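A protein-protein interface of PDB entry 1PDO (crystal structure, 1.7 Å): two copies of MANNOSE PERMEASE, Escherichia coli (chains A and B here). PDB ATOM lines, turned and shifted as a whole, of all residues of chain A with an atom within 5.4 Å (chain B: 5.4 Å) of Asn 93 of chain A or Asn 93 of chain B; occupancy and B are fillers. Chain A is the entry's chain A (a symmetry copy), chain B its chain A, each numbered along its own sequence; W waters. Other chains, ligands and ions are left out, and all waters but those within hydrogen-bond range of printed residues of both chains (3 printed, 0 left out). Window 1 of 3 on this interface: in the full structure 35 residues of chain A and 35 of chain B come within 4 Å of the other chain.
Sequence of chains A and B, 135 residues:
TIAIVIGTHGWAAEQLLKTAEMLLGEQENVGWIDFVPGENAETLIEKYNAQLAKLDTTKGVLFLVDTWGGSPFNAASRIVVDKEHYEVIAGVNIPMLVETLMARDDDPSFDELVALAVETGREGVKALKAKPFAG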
ATOM      1  N   GLY A  91      10.616 -12.892  17.411  1.00  0.00           N
ATOM      2  CA  GLY A  91      10.823 -14.193  18.003  1.00  0.00           C
ATOM      3  C   GLY A  91      12.048 -14.914  17.526  1.00  0.00           C
ATOM      4  O   GLY A  91      12.123 -16.131  17.609  1.00  0.00           O
ATOM      5  N   VAL A  92      13.042 -14.172  17.052  1.00  0.00           N
ATOM      6  CA  VAL A  92      14.256 -14.783  16.553  1.00  0.00           C
ATOM      7  C   VAL A  92      14.855 -15.838  17.515  1.00  0.00           C
ATOM      8  O   VAL A  92      14.986 -15.594  18.733  1.00  0.00           O
ATOM      9  CB  VAL A  92      15.327 -13.683  16.197  1.00  0.00           C
ATOM     10  CG1 VAL A  92      15.806 -12.937  17.455  1.00  0.00           C
ATOM     11  CG2 VAL A  92      16.508 -14.328  15.469  1.00  0.00           C
ATOM     12  N   ASN A  93      15.214 -16.998  16.972  1.00  0.00           N
ATOM     13  CA  ASN A  93      15.822 -18.067  17.756  1.00  0.00           C
ATOM     14  C   ASN A  93      16.884 -18.718  16.903  1.00  0.00           C
ATOM     15  O   ASN A  93      17.011 -18.392  15.713  1.00  0.00           O
ATOM     16  CB  ASN A  93      14.791 -19.075  18.341  1.00  0.00           C
ATOM     17  CG  ASN A  93      13.963 -19.751  17.296  1.00  0.00           C
ATOM     18  OD1 ASN A  93      14.283 -19.702  16.111  1.00  0.00           O
ATOM     19  ND2 ASN A  93      12.911 -20.449  17.723  1.00  0.00           N
ATOM     20  N   ILE A  94      17.704 -19.577  17.496  1.00  0.00           N
ATOM     21  CA  ILE A  94      18.760 -20.217  16.726  1.00  0.00           C
ATOM     22  C   ILE A  94      18.266 -21.065  15.546  1.00  0.00           C
ATOM     23  O   ILE A  94      18.853 -20.994  14.456  1.00  0.00           O
ATOM     24  CB  ILE A  94      19.807 -20.959  17.601  1.00  0.00           C
ATOM     25  CG1 ILE A  94      20.517 -19.945  18.534  1.00  0.00           C
ATOM     26  CG2 ILE A  94      20.868 -21.578  16.710  1.00  0.00           C
ATOM     27  CD1 ILE A  94      21.296 -18.865  17.779  1.00  0.00           C
ATOM     28  N   PRO A  95      17.195 -21.881  15.731  1.00  0.00           N
ATOM     29  CA  PRO A  95      16.729 -22.677  14.567  1.00  0.00           C
ATOM     30  C   PRO A  95      16.374 -21.741  13.380  1.00  0.00           C
ATOM     31  O   PRO A  95      16.767 -22.003  12.227  1.00  0.00           O
ATOM     32  CB  PRO A  95      15.476 -23.382  15.113  1.00  0.00           C
ATOM     33  CG  PRO A  95      15.846 -23.618  16.557  1.00  0.00           C
ATOM     34  CD  PRO A  95      16.475 -22.283  16.964  1.00  0.00           C
ATOM     35  N   MET A  96      15.692 -20.633  13.664  1.00  0.00           N
ATOM     36  CA  MET A  96      15.340 -19.696  12.608  1.00  0.00           C
ATOM     37  C   MET A  96      16.617 -19.142  11.959  1.00  0.00           C
ATOM     38  O   MET A  96      16.712 -19.075  10.748  1.00  0.00           O
ATOM     39  CB  MET A  96      14.545 -18.516  13.181  1.00  0.00           C
ATOM     40  CG  MET A  96      14.170 -17.391  12.142  1.00  0.00           C
ATOM     41  SD  MET A  96      13.494 -15.826  12.794  1.00  0.00           S
ATOM     42  CE  MET A  96      11.928 -16.503  13.711  1.00  0.00           C
ATOM     43  N   LEU A  97      17.571 -18.683  12.773  1.00  0.00           N
ATOM     44  CA  LEU A  97      18.786 -18.093  12.225  1.00  0.00           C
ATOM     45  C   LEU A  97      19.578 -19.069  11.355  1.00  0.00           C
ATOM     46  O   LEU A  97      19.989 -18.737  10.277  1.00  0.00           O
ATOM     47  CB  LEU A  97      19.632 -17.535  13.375  1.00  0.00           C
ATOM     48  CG  LEU A  97      20.717 -16.502  13.066  1.00  0.00           C
ATOM     49  CD1 LEU A  97      20.133 -15.300  12.317  1.00  0.00           C
ATOM     50  CD2 LEU A  97      21.342 -16.059  14.369  1.00  0.00           C
ATOM     51  N   VAL A  98      19.798 -20.275  11.845  1.00  0.00           N
ATOM     52  CA  VAL A  98      20.536 -21.296  11.133  1.00  0.00           C
ATOM     53  C   VAL A  98      19.865 -21.696   9.796  1.00  0.00           C
ATOM     54  O   VAL A  98      20.523 -21.744   8.753  1.00  0.00           O
ATOM     55  CB  VAL A  98      20.735 -22.528  12.072  1.00  0.00           C
ATOM     56  CG1 VAL A  98      21.265 -23.728  11.326  1.00  0.00           C
ATOM     57  CG2 VAL A  98      21.703 -22.148  13.193  1.00  0.00           C
ATOM     58  N   THR A 120      10.533 -22.319  10.254  1.00  0.00           N
ATOM     59  CA  THR A 120      11.608 -22.983  10.995  1.00  0.00           C
ATOM     60  C   THR A 120      11.731 -22.451  12.419  1.00  0.00           C
ATOM     61  O   THR A 120      12.103 -23.181  13.318  1.00  0.00           O
ATOM     62  CB  THR A 120      12.974 -22.891  10.282  1.00  0.00           C
ATOM     63  OG1 THR A 120      13.324 -21.509  10.074  1.00  0.00           O
ATOM     64  CG2 THR A 120      12.890 -23.597   8.931  1.00  0.00           C
ATOM     65  N   GLY A 121      11.427 -21.167  12.604  1.00  0.00           N
ATOM     66  CA  GLY A 121      11.467 -20.571  13.935  1.00  0.00           C
ATOM     67  C   GLY A 121      10.448 -21.265  14.831  1.00  0.00           C
ATOM     68  O   GLY A 121      10.751 -21.640  15.957  1.00  0.00           O
ATOM     69  N   ARG A 122       9.244 -21.463  14.313  1.00  0.00           N
ATOM     70  CA  ARG A 122       8.168 -22.105  15.075  1.00  0.00           C
ATOM     71  C   ARG A 122       8.392 -23.589  15.258  1.00  0.00           C
ATOM     72  O   ARG A 122       8.169 -24.123  16.325  1.00  0.00           O
ATOM     73  CB  ARG A 122       6.812 -21.893  14.385  1.00  0.00           C
ATOM     74  CG  ARG A 122       6.283 -20.481  14.489  1.00  0.00           C
ATOM     75  CD  ARG A 122       4.996 -20.302  13.684  1.00  0.00           C
ATOM     76  NE  ARG A 122       4.542 -18.909  13.672  1.00  0.00           N
ATOM     77  CZ  ARG A 122       3.646 -18.416  12.819  1.00  0.00           C
ATOM     78  NH1 ARG A 122       3.097 -19.206  11.902  1.00  0.00           N
ATOM     79  NH2 ARG A 122       3.335 -17.122  12.848  1.00  0.00           N
ATOM     80  N   GLY A 124      11.111 -25.031  15.396  1.00  0.00           N
ATOM     81  CA  GLY A 124      12.282 -25.218  16.245  1.00  0.00           C
ATOM     82  C   GLY A 124      11.950 -25.276  17.740  1.00  0.00           C
ATOM     83  O   GLY A 124      12.792 -25.683  18.538  1.00  0.00           O
ATOM     84  N   VAL A 125      10.757 -24.821  18.119  1.00  0.00           N
ATOM     85  CA  VAL A 125      10.340 -24.838  19.529  1.00  0.00           C
ATOM     86  C   VAL A 125       9.672 -26.195  19.760  1.00  0.00           C
ATOM     87  O   VAL A 125       8.577 -26.475  19.252  1.00  0.00           O
ATOM     88  CB  VAL A 125       9.397 -23.689  19.832  1.00  0.00           C
ATOM     89  CG1 VAL A 125       8.896 -23.785  21.261  1.00  0.00           C
ATOM     90  CG2 VAL A 125      10.107 -22.357  19.571  1.00  0.00           C
ATOM     91  N   GLY B  91      14.716 -24.284  21.017  1.00  0.00           N
ATOM     92  CA  GLY B  91      14.236 -23.116  20.317  1.00  0.00           C
ATOM     93  C   GLY B  91      13.998 -21.915  21.183  1.00  0.00           C
ATOM     94  O   GLY B  91      13.230 -21.036  20.827  1.00  0.00           O
ATOM     95  N   VAL B  92      14.682 -21.845  22.321  1.00  0.00           N
ATOM     96  CA  VAL B  92      14.503 -20.731  23.229  1.00  0.00           C
ATOM     97  C   VAL B  92      14.577 -19.350  22.532  1.00  0.00           C
ATOM     98  O   VAL B  92      15.495 -19.085  21.728  1.00  0.00           O
ATOM     99  CB  VAL B  92      15.537 -20.811  24.417  1.00  0.00           C
ATOM    100  CG1 VAL B  92      16.982 -20.624  23.918  1.00  0.00           C
ATOM    101  CG2 VAL B  92      15.191 -19.761  25.474  1.00  0.00           C
ATOM    102  N   ASN B  93      13.616 -18.481  22.838  1.00  0.00           N
ATOM    103  CA  ASN B  93      13.582 -17.134  22.279  1.00  0.00           C
ATOM    104  C   ASN B  93      13.108 -16.198  23.366  1.00  0.00           C
ATOM    105  O   ASN B  93      12.716 -16.653  24.451  1.00  0.00           O
ATOM    106  CB  ASN B  93      12.761 -17.025  20.964  1.00  0.00           C
ATOM    107  CG  ASN B  93      11.333 -17.443  21.118  1.00  0.00           C
ATOM    108  OD1 ASN B  93      10.835 -17.578  22.233  1.00  0.00           O
ATOM    109  ND2 ASN B  93      10.629 -17.597  19.997  1.00  0.00           N
ATOM    110  N   ILE B  94      13.206 -14.895  23.135  1.00  0.00           N
ATOM    111  CA  ILE B  94      12.784 -13.946  24.156  1.00  0.00           C
ATOM    112  C   ILE B  94      11.306 -14.055  24.556  1.00  0.00           C
ATOM    113  O   ILE B  94      10.994 -13.993  25.755  1.00  0.00           O
ATOM    114  CB  ILE B  94      13.222 -12.484  23.868  1.00  0.00           C
ATOM    115  CG1 ILE B  94      14.768 -12.404  23.826  1.00  0.00           C
ATOM    116  CG2 ILE B  94      12.748 -11.581  24.990  1.00  0.00           C
ATOM    117  CD1 ILE B  94      15.434 -12.784  25.151  1.00  0.00           C
ATOM    118  N   PRO B  95      10.374 -14.211  23.581  1.00  0.00           N
ATOM    119  CA  PRO B  95       8.955 -14.329  24.000  1.00  0.00           C
ATOM    120  C   PRO B  95       8.777 -15.523  24.976  1.00  0.00           C
ATOM    121  O   PRO B  95       8.112 -15.393  26.022  1.00  0.00           O
ATOM    122  CB  PRO B  95       8.225 -14.586  22.670  1.00  0.00           C
ATOM    123  CG  PRO B  95       9.042 -13.774  21.694  1.00  0.00           C
ATOM    124  CD  PRO B  95      10.479 -14.106  22.104  1.00  0.00           C
ATOM    125  N   MET B  96       9.413 -16.654  24.674  1.00  0.00           N
ATOM    126  CA  MET B  96       9.312 -17.810  25.550  1.00  0.00           C
ATOM    127  C   MET B  96       9.889 -17.465  26.932  1.00  0.00           C
ATOM    128  O   MET B  96       9.289 -17.777  27.944  1.00  0.00           O
ATOM    129  CB  MET B  96      10.112 -18.987  24.980  1.00  0.00           C
ATOM    130  CG  MET B  96      10.142 -20.280  25.882  1.00  0.00           C
ATOM    131  SD  MET B  96      11.308 -21.608  25.424  1.00  0.00           S
ATOM    132  CE  MET B  96      10.671 -21.998  23.637  1.00  0.00           C
ATOM    133  N   LEU B  97      11.088 -16.880  26.969  1.00  0.00           N
ATOM    134  CA  LEU B  97      11.720 -16.574  28.246  1.00  0.00           C
ATOM    135  C   LEU B  97      10.892 -15.615  29.103  1.00  0.00           C
ATOM    136  O   LEU B  97      10.691 -15.846  30.264  1.00  0.00           O
ATOM    137  CB  LEU B  97      13.132 -16.037  27.989  1.00  0.00           C
ATOM    138  CG  LEU B  97      14.151 -16.050  29.129  1.00  0.00           C
ATOM    139  CD1 LEU B  97      14.308 -17.459  29.710  1.00  0.00           C
ATOM    140  CD2 LEU B  97      15.474 -15.548  28.595  1.00  0.00           C
ATOM    141  N   VAL B  98      10.426 -14.529  28.515  1.00  0.00           N
ATOM    142  CA  VAL B  98       9.632 -13.535  29.205  1.00  0.00           C
ATOM    143  C   VAL B  98       8.301 -14.106  29.751  1.00  0.00           C
ATOM    144  O   VAL B  98       7.963 -13.903  30.920  1.00  0.00           O
ATOM    145  CB  VAL B  98       9.395 -12.322  28.251  1.00  0.00           C
ATOM    146  CG1 VAL B  98       8.366 -11.363  28.800  1.00  0.00           C
ATOM    147  CG2 VAL B  98      10.719 -11.590  28.036  1.00  0.00           C
ATOM    148  N   THR B 120       4.043 -20.073  23.924  1.00  0.00           N
ATOM    149  CA  THR B 120       4.472 -18.680  23.777  1.00  0.00           C
ATOM    150  C   THR B 120       5.705 -18.555  22.890  1.00  0.00           C
ATOM    151  O   THR B 120       5.869 -17.564  22.202  1.00  0.00           O
ATOM    152  CB  THR B 120       4.728 -17.985  25.131  1.00  0.00           C
ATOM    153  OG1 THR B 120       5.727 -18.713  25.871  1.00  0.00           O
ATOM    154  CG2 THR B 120       3.432 -17.949  25.937  1.00  0.00           C
ATOM    155  N   GLY B 121       6.572 -19.565  22.926  1.00  0.00           N
ATOM    156  CA  GLY B 121       7.761 -19.566  22.081  1.00  0.00           C
ATOM    157  C   GLY B 121       7.341 -19.570  20.616  1.00  0.00           C
ATOM    158  O   GLY B 121       7.851 -18.800  19.812  1.00  0.00           O
ATOM    159  N   ARG B 122       6.381 -20.421  20.280  1.00  0.00           N
ATOM    160  CA  ARG B 122       5.896 -20.536  18.901  1.00  0.00           C
ATOM    161  C   ARG B 122       5.063 -19.348  18.477  1.00  0.00           C
ATOM    162  O   ARG B 122       5.200 -18.855  17.376  1.00  0.00           O
ATOM    163  CB  ARG B 122       5.058 -21.812  18.724  1.00  0.00           C
ATOM    164  CG  ARG B 122       5.870 -23.087  18.733  1.00  0.00           C
ATOM    165  CD  ARG B 122       4.975 -24.324  18.675  1.00  0.00           C
ATOM    166  NE  ARG B 122       5.741 -25.566  18.810  1.00  0.00           N
ATOM    167  CZ  ARG B 122       5.207 -26.752  19.099  1.00  0.00           C
ATOM    168  NH1 ARG B 122       3.896 -26.864  19.280  1.00  0.00           N
ATOM    169  NH2 ARG B 122       5.991 -27.817  19.256  1.00  0.00           N
ATOM    170  N   GLY B 124       5.327 -16.460  19.517  1.00  0.00           N
ATOM    171  CA  GLY B 124       6.190 -15.286  19.472  1.00  0.00           C
ATOM    172  C   GLY B 124       6.853 -15.067  18.109  1.00  0.00           C
ATOM    173  O   GLY B 124       7.391 -13.990  17.855  1.00  0.00           O
ATOM    174  N   VAL B 125       6.864 -16.095  17.263  1.00  0.00           N
ATOM    175  CA  VAL B 125       7.470 -15.987  15.927  1.00  0.00           C
ATOM    176  C   VAL B 125       6.363 -15.490  14.994  1.00  0.00           C
ATOM    177  O   VAL B 125       5.400 -16.208  14.689  1.00  0.00           O
ATOM    178  CB  VAL B 125       8.031 -17.321  15.473  1.00  0.00           C
ATOM    179  CG1 VAL B 125       8.557 -17.213  14.052  1.00  0.00           C
ATOM    180  CG2 VAL B 125       9.122 -17.779  16.445  1.00  0.00           C
HETATM  181  O   HOH W   1      17.327 -16.328  21.055  1.00  0.00           O
HETATM  182  O   HOH W   2      17.237 -20.741  20.104  1.00  0.00           O
HETATM  183  O   HOH W   3      13.671 -13.731  20.526  1.00  0.00           O
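Asn 93 of chain A touches just these residues of chain B: Gly 91 (3.2 Å), Val 92 (3.5 Å) and Asn 93 (3.9 Å). Asn 93 of chain B touches just these residues of chain A: Gly 91 (3.2 Å), Val 92 (3.5 Å) and Asn 93 (3.9 Å). Of the printed residues of chain B, Gly 91 of chain A touches Asn 93 (3.2 Å), Gly 124 (3.4 Å) and Val 125 (3.6 Å). Of the printed residues of chain A, Met 96 of chain B touches Val 125 (3.5 Å). Printed residues of chain B within 4 Å of Val 92 of chain A: Asn 93. Printed residues of chain B within 4 Å of Met 96 of chain A: Val 125. Printed residues of chain A within 4 Å of Val 92 of chain B: Asn 93 (3.5 Å). Val 98 of chain A touches none of the printed residues of chain B. Ile 94 of chain A touches none of the printed residues of chain B. The nearest residue of chain B that does not touch Asn 93 of chain A is Val 125 of chain B (4.8 Å).
The side-chain amide oxygen (OD1) of Asn 93 of chain B is in hydrogen-bond range of the backbone NH (N) of Met 96 of chain B. The side-chain amide nitrogen (ND2) of Asn 93 of chain B sits at hydrogen-bond distance from the backbone carbonyl oxygen (O) of Gly 121 of chain B, at 3.0 Å. N of Met 96 of chain A lies within hydrogen-bond range of OD1 of Asn 93 of chain A, 3.0 Å away. The side-chain amide nitrogen (ND2) of Asn 93 of chain A lies within hydrogen-bond range of the backbone carbonyl oxygen (O) of Gly 121 of chain A.
Water W2 bridges N of Ile 94 of chain A and O of Val 92 of chain B. Water W3 bridges the backbone NH of Ile 94 of chain B and the backbone carbonyl oxygen of Val 92 of chain A. Water W1 bridges O of Val 92 of chain B (3.4 Å) and O of Val 92 of chain A (3.4 Å).
Val 125 of chain B touches Gly 91 of chain A. Val 92 of chain A touches Asn 93 of chain B. Val 92 of chain B touches Asn 93 of chain A (O to CB, 3.5 Å). Asn 93 of chain A touches Asn 93 of chain B (CB to CB, 3.9 Å). CE of Met 96 of chain A touches CG1 of Val 125 of chain B, 3.5 Å away. Arg 122 of chain A touches Arg 122 of chain B (CG to O, 3.5 Å). Val 125 of chain A touches Gly 91 of chain B (CG2 to O, 3.6 Å). CE of Met 96 of chain B touches CG1 of Val 125 of chain A, 3.5 Å away.
Of the 13 printed residues of chain A, 7 touch a printed residue of chain B. Hydrophobic or aromatic side chains of chain A that line the printed part of chain B: Met 96 and Val 125. Along chain A the printed residues that touch a printed residue of chain B span positions 91 to 125. Among the printed residues, no Asp or Glu carboxylate lies within 4 Å of a Lys or Arg side-chain nitrogen of the other chain.
The side-chain amide nitrogen of Asn 93 of chain A is in hydrogen-bond range of the backbone carbonyl oxygen of Gly 91 of chain B (3.2 Å). N of Gly 91 of chain B is in hydrogen-bond range of O of Gly 124 of chain A. ND2 of Asn 93 of chain B is in hydrogen-bond range of O of Gly 91 of chain A, 3.2 Å away. The guanidinium group (NH2) of Arg 122 of chain B is in hydrogen-bond range of the backbone carbonyl oxygen (O) of Val 125 of chain A (2.9 Å). The backbone NH (N) of Gly 91 of chain A sits at hydrogen-bond distance from the backbone carbonyl oxygen (O) of Gly 124 of chain B (3.4 Å). The backbone carbonyl oxygen of Val 125 of chain B is in hydrogen-bond range of the guanidinium group of Arg 122 of chain A, at 2.9 Å.
Val 92 of chain A touches Asn 93 of chain B, and with the chains exchanged Asn 93 of chain A touches Val 92 of chain B. Met 96 of chain A touches Val 125 of chain B, and with the chains exchanged Val 125 of chain A touches Met 96 of chain B. Arg 122 of chain A touches its own counterpart, Arg 122 of chain B. Arg 122 of chain A touches Val 125 of chain B, and with the chains exchanged Val 125 of chain A touches Arg 122 of chain B. Positions printed for both chains: 91, 92, 93, 94, 95, 96, 97, 98, 120, 121, 122, 124 and 125.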
